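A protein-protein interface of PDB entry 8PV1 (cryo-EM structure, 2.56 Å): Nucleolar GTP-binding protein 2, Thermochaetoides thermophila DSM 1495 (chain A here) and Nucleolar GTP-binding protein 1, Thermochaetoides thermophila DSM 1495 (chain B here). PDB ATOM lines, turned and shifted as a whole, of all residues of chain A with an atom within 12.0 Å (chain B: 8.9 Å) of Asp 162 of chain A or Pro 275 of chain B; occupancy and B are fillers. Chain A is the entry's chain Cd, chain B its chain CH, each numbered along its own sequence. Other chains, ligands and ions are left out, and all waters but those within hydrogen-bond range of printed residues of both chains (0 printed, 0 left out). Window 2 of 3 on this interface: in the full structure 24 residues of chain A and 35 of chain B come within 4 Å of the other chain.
Of the 18 printed residues of chain B, 5 touch a printed residue of chain A. Of the 16 printed residues of chain A, 6 touch a printed residue of chain B. Hydrophobic or aromatic side chains of chain A that line the printed part of chain B: Phe 158, Val 161, Leu 164 and Ala 165. Among the printed residues, 12 pairs touch across the chains.
The side-chain hydroxyl (OG1) of Thr 160 of chain A sits close to the backbone NH (N) of Asp 162 of chain A, at 3.5 Å. O of Leu 164 of chain A sits at hydrogen-bond distance from OG of Ser 168 of chain A, at 3.1 Å. OG of Ser 168 of chain A is in hydrogen-bond range of O of Ala 165 of chain A, 2.6 Å away.
Of chain B, only Pro 275 (3.4 Å) comes within 4 Å of Asp 162 of chain A. Pro 275 of chain B touches just these residues of chain A: Val 161, Asp 162 and Ala 165. Val 161 of chain A touches just these residues of chain B: Leu 228 (3.7 Å), Ser 272 (3.5 Å), Pro 275 (3.7 Å) and Leu 276 (3.7 Å). No residue of chain A comes within 4 Å of Ile 273 of chain B. No residue of chain A comes within 4 Å of Lys 274 of chain B. No residue of chain A comes within 4 Å of Phe 277 of chain B. No residue of chain A comes within 4 Å of Ala 278 of chain B. Printed residues of chain A within 4 Å of Ala 243 of chain B: Leu 164 and Ser 168. Printed residues of chain B within 4 Å of Ser 168 of chain A: Ala 243. Of the printed residues of chain B, Leu 164 of chain A touches Leu 228, Ala 243 and Leu 276. Thr 160 of chain A touches none of the printed residues of chain B. The nearest residue of chain B that does not touch Asp 162 of chain A is Leu 276 of chain B (5.9 Å). The nearest residue of chain A that does not touch Pro 275 of chain B is Gly 166 of chain A (7.0 Å). The nearest printed residue of chain B that does not touch Ala 165 of chain A is Ala 243 of chain B (5.9 Å).
Among the printed residues, pairs that only touch across the chains: Asp 162 of chain A with Pro 275 of chain B (3.4 Å), Val 161 of chain A with Ser 272 of chain B (3.5 Å), Ser 168 of chain A with Ala 243 of chain B (3.6 Å), Val 161 of chain A with Leu 276 of chain B (3.7 Å), Val 161 of chain A with Pro 275 of chain B (3.7 Å), Phe 158 of chain A with Leu 228 of chain B (3.7 Å), Leu 164 of chain A with Leu 276 of chain B (3.7 Å), Val 161 of chain A with Leu 228 of chain B (3.7 Å), Leu 164 of chain A with Ala 243 of chain B (3.8 Å), Leu 164 of chain A with Leu 228 of chain B (3.9 Å), Ala 165 of chain A with Pro 275 of chain B (3.97 Å) and Ala 165 of chain A with Leu 276 of chain B (3.998 Å).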
ATOM      1  N   LEU A 156     -22.401   2.024  14.001  1.00  0.00           N
ATOM      2  CA  LEU A 156     -22.004   0.680  14.381  1.00  0.00           C
ATOM      3  C   LEU A 156     -22.180  -0.275  13.208  1.00  0.00           C
ATOM      4  O   LEU A 156     -23.068  -0.107  12.367  1.00  0.00           O
ATOM      5  CB  LEU A 156     -22.816   0.184  15.582  1.00  0.00           C
ATOM      6  CG  LEU A 156     -22.876   1.136  16.777  1.00  0.00           C
ATOM      7  CD1 LEU A 156     -23.891   0.655  17.797  1.00  0.00           C
ATOM      8  CD2 LEU A 156     -21.506   1.286  17.404  1.00  0.00           C
ATOM      9  N   SER A 157     -21.315  -1.286  13.162  1.00  0.00           N
ATOM     10  CA  SER A 157     -21.391  -2.346  12.168  1.00  0.00           C
ATOM     11  C   SER A 157     -22.199  -3.538  12.659  1.00  0.00           C
ATOM     12  O   SER A 157     -22.255  -4.563  11.974  1.00  0.00           O
ATOM     13  CB  SER A 157     -19.985  -2.796  11.770  1.00  0.00           C
ATOM     14  OG  SER A 157     -19.216  -3.123  12.914  1.00  0.00           O
ATOM     15  N   PHE A 158     -22.819  -3.424  13.829  1.00  0.00           N
ATOM     16  CA  PHE A 158     -23.591  -4.501  14.425  1.00  0.00           C
ATOM     17  C   PHE A 158     -24.919  -3.939  14.905  1.00  0.00           C
ATOM     18  O   PHE A 158     -25.039  -2.750  15.206  1.00  0.00           O
ATOM     19  CB  PHE A 158     -22.832  -5.163  15.586  1.00  0.00           C
ATOM     20  CG  PHE A 158     -22.137  -4.184  16.492  1.00  0.00           C
ATOM     21  CD1 PHE A 158     -22.816  -3.587  17.541  1.00  0.00           C
ATOM     22  CD2 PHE A 158     -20.802  -3.867  16.300  1.00  0.00           C
ATOM     23  CE1 PHE A 158     -22.183  -2.686  18.372  1.00  0.00           C
ATOM     24  CE2 PHE A 158     -20.165  -2.966  17.127  1.00  0.00           C
ATOM     25  CZ  PHE A 158     -20.855  -2.374  18.164  1.00  0.00           C
ATOM     26  N   ASN A 159     -25.922  -4.811  14.971  1.00  0.00           N
ATOM     27  CA  ASN A 159     -27.248  -4.416  15.420  1.00  0.00           C
ATOM     28  C   ASN A 159     -27.727  -5.170  16.649  1.00  0.00           C
ATOM     29  O   ASN A 159     -28.555  -4.632  17.393  1.00  0.00           O
ATOM     30  CB  ASN A 159     -28.275  -4.603  14.293  1.00  0.00           C
ATOM     31  CG  ASN A 159     -28.126  -3.573  13.193  1.00  0.00           C
ATOM     32  OD1 ASN A 159     -27.474  -3.821  12.178  1.00  0.00           O
ATOM     33  ND2 ASN A 159     -28.729  -2.407  13.390  1.00  0.00           N
ATOM     34  N   THR A 160     -27.243  -6.386  16.886  1.00  0.00           N
ATOM     35  CA  THR A 160     -27.680  -7.190  18.015  1.00  0.00           C
ATOM     36  C   THR A 160     -26.489  -7.533  18.899  1.00  0.00           C
ATOM     37  O   THR A 160     -25.329  -7.346  18.525  1.00  0.00           O
ATOM     38  CB  THR A 160     -28.376  -8.490  17.571  1.00  0.00           C
ATOM     39  OG1 THR A 160     -27.395  -9.426  17.109  1.00  0.00           O
ATOM     40  CG2 THR A 160     -29.380  -8.223  16.459  1.00  0.00           C
ATOM     41  N   VAL A 161     -26.810  -8.046  20.088  1.00  0.00           N
ATOM     42  CA  VAL A 161     -25.784  -8.431  21.053  1.00  0.00           C
ATOM     43  C   VAL A 161     -24.990  -9.629  20.542  1.00  0.00           C
ATOM     44  O   VAL A 161     -23.769  -9.714  20.731  1.00  0.00           O
ATOM     45  CB  VAL A 161     -26.444  -8.708  22.418  1.00  0.00           C
ATOM     46  CG1 VAL A 161     -25.428  -9.163  23.436  1.00  0.00           C
ATOM     47  CG2 VAL A 161     -27.169  -7.469  22.911  1.00  0.00           C
ATOM     48  N   ASP A 162     -25.669 -10.569  19.874  1.00  0.00           N
ATOM     49  CA  ASP A 162     -24.978 -11.712  19.282  1.00  0.00           C
ATOM     50  C   ASP A 162     -24.033 -11.275  18.168  1.00  0.00           C
ATOM     51  O   ASP A 162     -22.910 -11.789  18.055  1.00  0.00           O
ATOM     52  CB  ASP A 162     -25.996 -12.722  18.755  1.00  0.00           C
ATOM     53  CG  ASP A 162     -26.763 -13.407  19.868  1.00  0.00           C
ATOM     54  OD1 ASP A 162     -26.201 -13.557  20.973  1.00  0.00           O
ATOM     55  OD2 ASP A 162     -27.927 -13.796  19.638  1.00  0.00           O
ATOM     56  N   GLU A 163     -24.473 -10.323  17.336  1.00  0.00           N
ATOM     57  CA  GLU A 163     -23.595  -9.764  16.315  1.00  0.00           C
ATOM     58  C   GLU A 163     -22.408  -9.047  16.936  1.00  0.00           C
ATOM     59  O   GLU A 163     -21.295  -9.136  16.412  1.00  0.00           O
ATOM     60  CB  GLU A 163     -24.363  -8.806  15.405  1.00  0.00           C
ATOM     61  CG  GLU A 163     -25.396  -9.470  14.518  1.00  0.00           C
ATOM     62  CD  GLU A 163     -26.225  -8.465  13.744  1.00  0.00           C
ATOM     63  OE1 GLU A 163     -26.077  -7.252  13.998  1.00  0.00           O
ATOM     64  OE2 GLU A 163     -27.022  -8.887  12.880  1.00  0.00           O
ATOM     65  N   LEU A 164     -22.624  -8.345  18.052  1.00  0.00           N
ATOM     66  CA  LEU A 164     -21.520  -7.682  18.738  1.00  0.00           C
ATOM     67  C   LEU A 164     -20.509  -8.689  19.273  1.00  0.00           C
ATOM     68  O   LEU A 164     -19.297  -8.476  19.162  1.00  0.00           O
ATOM     69  CB  LEU A 164     -22.059  -6.810  19.870  1.00  0.00           C
ATOM     70  CG  LEU A 164     -21.048  -6.100  20.773  1.00  0.00           C
ATOM     71  CD1 LEU A 164     -20.018  -5.318  19.975  1.00  0.00           C
ATOM     72  CD2 LEU A 164     -21.775  -5.192  21.737  1.00  0.00           C
ATOM     73  N   ALA A 165     -20.989  -9.793  19.851  1.00  0.00           N
ATOM     74  CA  ALA A 165     -20.082 -10.810  20.380  1.00  0.00           C
ATOM     75  C   ALA A 165     -19.274 -11.472  19.267  1.00  0.00           C
ATOM     76  O   ALA A 165     -18.050 -11.646  19.391  1.00  0.00           O
ATOM     77  CB  ALA A 165     -20.872 -11.854  21.165  1.00  0.00           C
ATOM     78  N   GLY A 166     -19.942 -11.835  18.167  1.00  0.00           N
ATOM     79  CA  GLY A 166     -19.231 -12.419  17.040  1.00  0.00           C
ATOM     80  C   GLY A 166     -18.241 -11.456  16.411  1.00  0.00           C
ATOM     81  O   GLY A 166     -17.125 -11.843  16.051  1.00  0.00           O
ATOM     82  N   TYR A 167     -18.630 -10.184  16.293  1.00  0.00           N
ATOM     83  CA  TYR A 167     -17.739  -9.175  15.737  1.00  0.00           C
ATOM     84  C   TYR A 167     -16.530  -8.956  16.635  1.00  0.00           C
ATOM     85  O   TYR A 167     -15.412  -8.778  16.142  1.00  0.00           O
ATOM     86  CB  TYR A 167     -18.514  -7.873  15.525  1.00  0.00           C
ATOM     87  CG  TYR A 167     -17.661  -6.630  15.444  1.00  0.00           C
ATOM     88  CD1 TYR A 167     -16.988  -6.309  14.274  1.00  0.00           C
ATOM     89  CD2 TYR A 167     -17.551  -5.764  16.523  1.00  0.00           C
ATOM     90  CE1 TYR A 167     -16.214  -5.173  14.186  1.00  0.00           C
ATOM     91  CE2 TYR A 167     -16.777  -4.627  16.445  1.00  0.00           C
ATOM     92  CZ  TYR A 167     -16.112  -4.336  15.274  1.00  0.00           C
ATOM     93  OH  TYR A 167     -15.341  -3.201  15.190  1.00  0.00           O
ATOM     94  N   SER A 168     -16.730  -8.988  17.955  1.00  0.00           N
ATOM     95  CA  SER A 168     -15.619  -8.803  18.883  1.00  0.00           C
ATOM     96  C   SER A 168     -14.638  -9.968  18.816  1.00  0.00           C
ATOM     97  O   SER A 168     -13.417  -9.763  18.839  1.00  0.00           O
ATOM     98  CB  SER A 168     -16.148  -8.622  20.306  1.00  0.00           C
ATOM     99  OG  SER A 168     -16.951  -9.719  20.692  1.00  0.00           O
ATOM    100  N   GLU A 169     -15.146 -11.202  18.722  1.00  0.00           N
ATOM    101  CA  GLU A 169     -14.225 -12.339  18.675  1.00  0.00           C
ATOM    102  C   GLU A 169     -13.491 -12.402  17.334  1.00  0.00           C
ATOM    103  O   GLU A 169     -12.295 -12.724  17.288  1.00  0.00           O
ATOM    104  CB  GLU A 169     -14.956 -13.648  19.003  1.00  0.00           C
ATOM    105  CG  GLU A 169     -16.090 -14.086  18.091  1.00  0.00           C
ATOM    106  CD  GLU A 169     -15.619 -14.882  16.888  1.00  0.00           C
ATOM    107  OE1 GLU A 169     -14.491 -15.415  16.931  1.00  0.00           O
ATOM    108  OE2 GLU A 169     -16.386 -14.989  15.908  1.00  0.00           O
ATOM    109  N   GLN A 170     -14.174 -12.050  16.235  1.00  0.00           N
ATOM    110  CA  GLN A 170     -13.484 -11.959  14.948  1.00  0.00           C
ATOM    111  C   GLN A 170     -12.449 -10.838  14.941  1.00  0.00           C
ATOM    112  O   GLN A 170     -11.372 -10.986  14.352  1.00  0.00           O
ATOM    113  CB  GLN A 170     -14.481 -11.759  13.807  1.00  0.00           C
ATOM    114  CG  GLN A 170     -15.404 -12.933  13.555  1.00  0.00           C
ATOM    115  CD  GLN A 170     -16.506 -12.597  12.572  1.00  0.00           C
ATOM    116  OE1 GLN A 170     -17.689 -12.626  12.913  1.00  0.00           O
ATOM    117  NE2 GLN A 170     -16.123 -12.271  11.344  1.00  0.00           N
ATOM    118  N   SER A 171     -12.763  -9.706  15.581  1.00  0.00           N
ATOM    119  CA  SER A 171     -11.813  -8.602  15.664  1.00  0.00           C
ATOM    120  C   SER A 171     -10.580  -8.993  16.465  1.00  0.00           C
ATOM    121  O   SER A 171      -9.453  -8.647  16.090  1.00  0.00           O
ATOM    122  CB  SER A 171     -12.486  -7.380  16.285  1.00  0.00           C
ATOM    123  OG  SER A 171     -13.536  -6.902  15.465  1.00  0.00           O
ATOM    124  N   LEU B 228     -29.404  -1.685  20.875  1.00  0.00           N
ATOM    125  CA  LEU B 228     -28.163  -0.941  20.670  1.00  0.00           C
ATOM    126  C   LEU B 228     -28.322   0.188  19.660  1.00  0.00           C
ATOM    127  O   LEU B 228     -27.494   1.106  19.615  1.00  0.00           O
ATOM    128  CB  LEU B 228     -27.040  -1.882  20.226  1.00  0.00           C
ATOM    129  CG  LEU B 228     -26.316  -2.781  21.237  1.00  0.00           C
ATOM    130  CD1 LEU B 228     -27.174  -3.932  21.740  1.00  0.00           C
ATOM    131  CD2 LEU B 228     -25.025  -3.305  20.632  1.00  0.00           C
ATOM    132  N   LEU B 242     -17.663  -3.827  28.030  1.00  0.00           N
ATOM    133  CA  LEU B 242     -18.190  -5.162  28.295  1.00  0.00           C
ATOM    134  C   LEU B 242     -17.947  -6.115  27.131  1.00  0.00           C
ATOM    135  O   LEU B 242     -17.781  -7.319  27.346  1.00  0.00           O
ATOM    136  CB  LEU B 242     -19.684  -5.090  28.602  1.00  0.00           C
ATOM    137  CG  LEU B 242     -20.083  -4.424  29.918  1.00  0.00           C
ATOM    138  CD1 LEU B 242     -21.569  -4.125  29.924  1.00  0.00           C
ATOM    139  CD2 LEU B 242     -19.704  -5.299  31.095  1.00  0.00           C
ATOM    140  N   ALA B 243     -17.920  -5.603  25.903  1.00  0.00           N
ATOM    141  CA  ALA B 243     -17.818  -6.463  24.733  1.00  0.00           C
ATOM    142  C   ALA B 243     -16.390  -6.838  24.366  1.00  0.00           C
ATOM    143  O   ALA B 243     -16.176  -7.915  23.798  1.00  0.00           O
ATOM    144  CB  ALA B 243     -18.484  -5.792  23.530  1.00  0.00           C
ATOM    145  N   ASN B 268     -33.958  -7.803  33.085  1.00  0.00           N
ATOM    146  CA  ASN B 268     -34.082  -7.815  31.631  1.00  0.00           C
ATOM    147  C   ASN B 268     -32.814  -7.311  30.953  1.00  0.00           C
ATOM    148  O   ASN B 268     -32.382  -7.876  29.941  1.00  0.00           O
ATOM    149  CB  ASN B 268     -35.283  -6.976  31.198  1.00  0.00           C
ATOM    150  CG  ASN B 268     -36.608  -7.626  31.547  1.00  0.00           C
ATOM    151  OD1 ASN B 268     -36.675  -8.826  31.811  1.00  0.00           O
ATOM    152  ND2 ASN B 268     -37.673  -6.834  31.540  1.00  0.00           N
ATOM    153  N   LEU B 269     -32.201  -6.256  31.496  1.00  0.00           N
ATOM    154  CA  LEU B 269     -30.944  -5.761  30.944  1.00  0.00           C
ATOM    155  C   LEU B 269     -29.829  -6.784  31.116  1.00  0.00           C
ATOM    156  O   LEU B 269     -28.997  -6.966  30.216  1.00  0.00           O
ATOM    157  CB  LEU B 269     -30.558  -4.435  31.601  1.00  0.00           C
ATOM    158  CG  LEU B 269     -29.263  -3.824  31.051  1.00  0.00           C
ATOM    159  CD1 LEU B 269     -29.415  -3.470  29.578  1.00  0.00           C
ATOM    160  CD2 LEU B 269     -28.810  -2.622  31.851  1.00  0.00           C
ATOM    161  N   PHE B 270     -29.795  -7.460  32.270  1.00  0.00           N
ATOM    162  CA  PHE B 270     -28.797  -8.506  32.483  1.00  0.00           C
ATOM    163  C   PHE B 270     -28.959  -9.645  31.480  1.00  0.00           C
ATOM    164  O   PHE B 270     -27.974 -10.135  30.916  1.00  0.00           O
ATOM    165  CB  PHE B 270     -28.880  -9.037  33.913  1.00  0.00           C
ATOM    166  CG  PHE B 270     -27.852 -10.083  34.217  1.00  0.00           C
ATOM    167  CD1 PHE B 270     -26.538  -9.726  34.451  1.00  0.00           C
ATOM    168  CD2 PHE B 270     -28.197 -11.424  34.256  1.00  0.00           C
ATOM    169  CE1 PHE B 270     -25.587 -10.683  34.721  1.00  0.00           C
ATOM    170  CE2 PHE B 270     -27.247 -12.390  34.525  1.00  0.00           C
ATOM    171  CZ  PHE B 270     -25.940 -12.017  34.758  1.00  0.00           C
ATOM    172  N   LYS B 271     -30.201 -10.069  31.237  1.00  0.00           N
ATOM    173  CA  LYS B 271     -30.447 -11.119  30.250  1.00  0.00           C
ATOM    174  C   LYS B 271     -30.113 -10.646  28.841  1.00  0.00           C
ATOM    175  O   LYS B 271     -29.686 -11.442  27.996  1.00  0.00           O
ATOM    176  CB  LYS B 271     -31.900 -11.585  30.319  1.00  0.00           C
ATOM    177  CG  LYS B 271     -32.272 -12.324  31.589  1.00  0.00           C
ATOM    178  CD  LYS B 271     -33.725 -12.769  31.542  1.00  0.00           C
ATOM    179  CE  LYS B 271     -34.130 -13.494  32.811  1.00  0.00           C
ATOM    180  NZ  LYS B 271     -35.555 -13.921  32.772  1.00  0.00           N
ATOM    181  N   SER B 272     -30.315  -9.355  28.565  1.00  0.00           N
ATOM    182  CA  SER B 272     -30.008  -8.818  27.245  1.00  0.00           C
ATOM    183  C   SER B 272     -28.506  -8.792  26.988  1.00  0.00           C
ATOM    184  O   SER B 272     -28.053  -9.125  25.887  1.00  0.00           O
ATOM    185  CB  SER B 272     -30.601  -7.419  27.103  1.00  0.00           C
ATOM    186  OG  SER B 272     -30.138  -6.785  25.925  1.00  0.00           O
ATOM    187  N   ILE B 273     -27.713  -8.398  27.991  1.00  0.00           N
ATOM    188  CA  ILE B 273     -26.266  -8.310  27.809  1.00  0.00           C
ATOM    189  C   ILE B 273     -25.545  -9.594  28.195  1.00  0.00           C
ATOM    190  O   ILE B 273     -24.308  -9.630  28.155  1.00  0.00           O
ATOM    191  CB  ILE B 273     -25.664  -7.133  28.604  1.00  0.00           C
ATOM    192  CG1 ILE B 273     -25.786  -7.380  30.108  1.00  0.00           C
ATOM    193  CG2 ILE B 273     -26.337  -5.830  28.201  1.00  0.00           C
ATOM    194  CD1 ILE B 273     -25.436  -6.180  30.961  1.00  0.00           C
ATOM    195  N   LYS B 274     -26.278 -10.636  28.592  1.00  0.00           N
ATOM    196  CA  LYS B 274     -25.665 -11.938  28.852  1.00  0.00           C
ATOM    197  C   LYS B 274     -24.855 -12.540  27.697  1.00  0.00           C
ATOM    198  O   LYS B 274     -23.828 -13.178  27.992  1.00  0.00           O
ATOM    199  CB  LYS B 274     -26.746 -12.923  29.321  1.00  0.00           C
ATOM    200  CG  LYS B 274     -26.205 -14.106  30.105  1.00  0.00           C
ATOM    201  CD  LYS B 274     -27.271 -14.722  30.993  1.00  0.00           C
ATOM    202  CE  LYS B 274     -26.682 -15.803  31.882  1.00  0.00           C
ATOM    203  NZ  LYS B 274     -27.672 -16.311  32.872  1.00  0.00           N
ATOM    204  N   PRO B 275     -25.244 -12.445  26.409  1.00  0.00           N
ATOM    205  CA  PRO B 275     -24.359 -12.992  25.360  1.00  0.00           C
ATOM    206  C   PRO B 275     -22.981 -12.346  25.273  1.00  0.00           C
ATOM    207  O   PRO B 275     -22.044 -12.991  24.787  1.00  0.00           O
ATOM    208  CB  PRO B 275     -25.159 -12.764  24.072  1.00  0.00           C
ATOM    209  CG  PRO B 275     -26.553 -12.788  24.499  1.00  0.00           C
ATOM    210  CD  PRO B 275     -26.579 -12.142  25.847  1.00  0.00           C
ATOM    211  N   LEU B 276     -22.821 -11.100  25.723  1.00  0.00           N
ATOM    212  CA  LEU B 276     -21.492 -10.504  25.808  1.00  0.00           C
ATOM    213  C   LEU B 276     -20.654 -11.097  26.929  1.00  0.00           C
ATOM    214  O   LEU B 276     -19.434 -10.908  26.943  1.00  0.00           O
ATOM    215  CB  LEU B 276     -21.588  -8.992  26.019  1.00  0.00           C
ATOM    216  CG  LEU B 276     -22.220  -8.172  24.903  1.00  0.00           C
ATOM    217  CD1 LEU B 276     -22.169  -6.690  25.229  1.00  0.00           C
ATOM    218  CD2 LEU B 276     -21.536  -8.469  23.584  1.00  0.00           C
ATOM    219  N   PHE B 277     -21.280 -11.805  27.863  1.00  0.00           N
ATOM    220  CA  PHE B 277     -20.619 -12.272  29.074  1.00  0.00           C
ATOM    221  C   PHE B 277     -20.013 -13.659  28.918  1.00  0.00           C
ATOM    222  O   PHE B 277     -19.512 -14.210  29.903  1.00  0.00           O
ATOM    223  CB  PHE B 277     -21.611 -12.262  30.243  1.00  0.00           C
ATOM    224  CG  PHE B 277     -21.979 -10.881  30.743  1.00  0.00           C
ATOM    225  CD1 PHE B 277     -22.803 -10.741  31.847  1.00  0.00           C
ATOM    226  CD2 PHE B 277     -21.472  -9.731  30.150  1.00  0.00           C
ATOM    227  CE1 PHE B 277     -23.145  -9.493  32.324  1.00  0.00           C
ATOM    228  CE2 PHE B 277     -21.811  -8.481  30.622  1.00  0.00           C
ATOM    229  CZ  PHE B 277     -22.647  -8.362  31.712  1.00  0.00           C
ATOM    230  N   ALA B 278     -20.063 -14.237  27.720  1.00  0.00           N
ATOM    231  CA  ALA B 278     -19.426 -15.522  27.474  1.00  0.00           C
ATOM    232  C   ALA B 278     -17.911 -15.388  27.558  1.00  0.00           C
ATOM    233  O   ALA B 278     -17.346 -14.319  27.311  1.00  0.00           O
ATOM    234  CB  ALA B 278     -19.833 -16.067  26.107  1.00  0.00           C
ATOM    235  N   ASN B 279     -17.259 -16.492  27.933  1.00  0.00           N
ATOM    236  CA  ASN B 279     -15.823 -16.602  28.189  1.00  0.00           C
ATOM    237  C   ASN B 279     -15.346 -15.652  29.280  1.00  0.00           C
ATOM    238  O   ASN B 279     -14.166 -15.277  29.294  1.00  0.00           O
ATOM    239  CB  ASN B 279     -14.987 -16.382  26.921  1.00  0.00           C
ATOM    240  CG  ASN B 279     -15.371 -17.328  25.801  1.00  0.00           C
ATOM    241  OD1 ASN B 279     -15.886 -16.907  24.767  1.00  0.00           O
ATOM    242  ND2 ASN B 279     -15.122 -18.616  26.003  1.00  0.00           N
ATOM    243  N   LYS B 280     -16.228 -15.244  30.190  1.00  0.00           N
ATOM    244  CA  LYS B 280     -15.878 -14.378  31.305  1.00  0.00           C
ATOM    245  C   LYS B 280     -16.543 -14.915  32.561  1.00  0.00           C
ATOM    246  O   LYS B 280     -17.295 -15.890  32.518  1.00  0.00           O
ATOM    247  CB  LYS B 280     -16.310 -12.921  31.068  1.00  0.00           C
ATOM    248  CG  LYS B 280     -15.745 -12.292  29.807  1.00  0.00           C
ATOM    249  CD  LYS B 280     -16.240 -10.875  29.613  1.00  0.00           C
ATOM    250  CE  LYS B 280     -15.835 -10.355  28.246  1.00  0.00           C
ATOM    251  NZ  LYS B 280     -16.160  -8.914  28.082  1.00  0.00           N
ATOM    252  N   VAL B 282     -19.044 -13.783  35.792  1.00  0.00           N
ATOM    253  CA  VAL B 282     -20.093 -12.817  36.079  1.00  0.00           C
ATOM    254  C   VAL B 282     -20.474 -12.907  37.549  1.00  0.00           C
ATOM    255  O   VAL B 282     -20.809 -13.984  38.058  1.00  0.00           O
ATOM    256  CB  VAL B 282     -21.333 -13.036  35.190  1.00  0.00           C
ATOM    257  CG1 VAL B 282     -22.309 -11.897  35.376  1.00  0.00           C
ATOM    258  CG2 VAL B 282     -20.935 -13.164  33.737  1.00  0.00           C
ATOM    259  N   GLU B 313     -22.826 -20.238  36.112  1.00  0.00           N
ATOM    260  CA  GLU B 313     -21.812 -19.342  35.576  1.00  0.00           C
ATOM    261  C   GLU B 313     -21.795 -17.990  36.284  1.00  0.00           C
ATOM    262  O   GLU B 313     -20.768 -17.303  36.258  1.00  0.00           O
ATOM    263  CB  GLU B 313     -22.048 -19.188  34.059  1.00  0.00           C
ATOM    264  CG  GLU B 313     -20.968 -18.481  33.230  1.00  0.00           C
ATOM    265  CD  GLU B 313     -21.072 -16.971  33.237  1.00  0.00           C
ATOM    266  OE1 GLU B 313     -22.195 -16.451  33.388  1.00  0.00           O
ATOM    267  OE2 GLU B 313     -20.032 -16.303  33.084  1.00  0.00           O
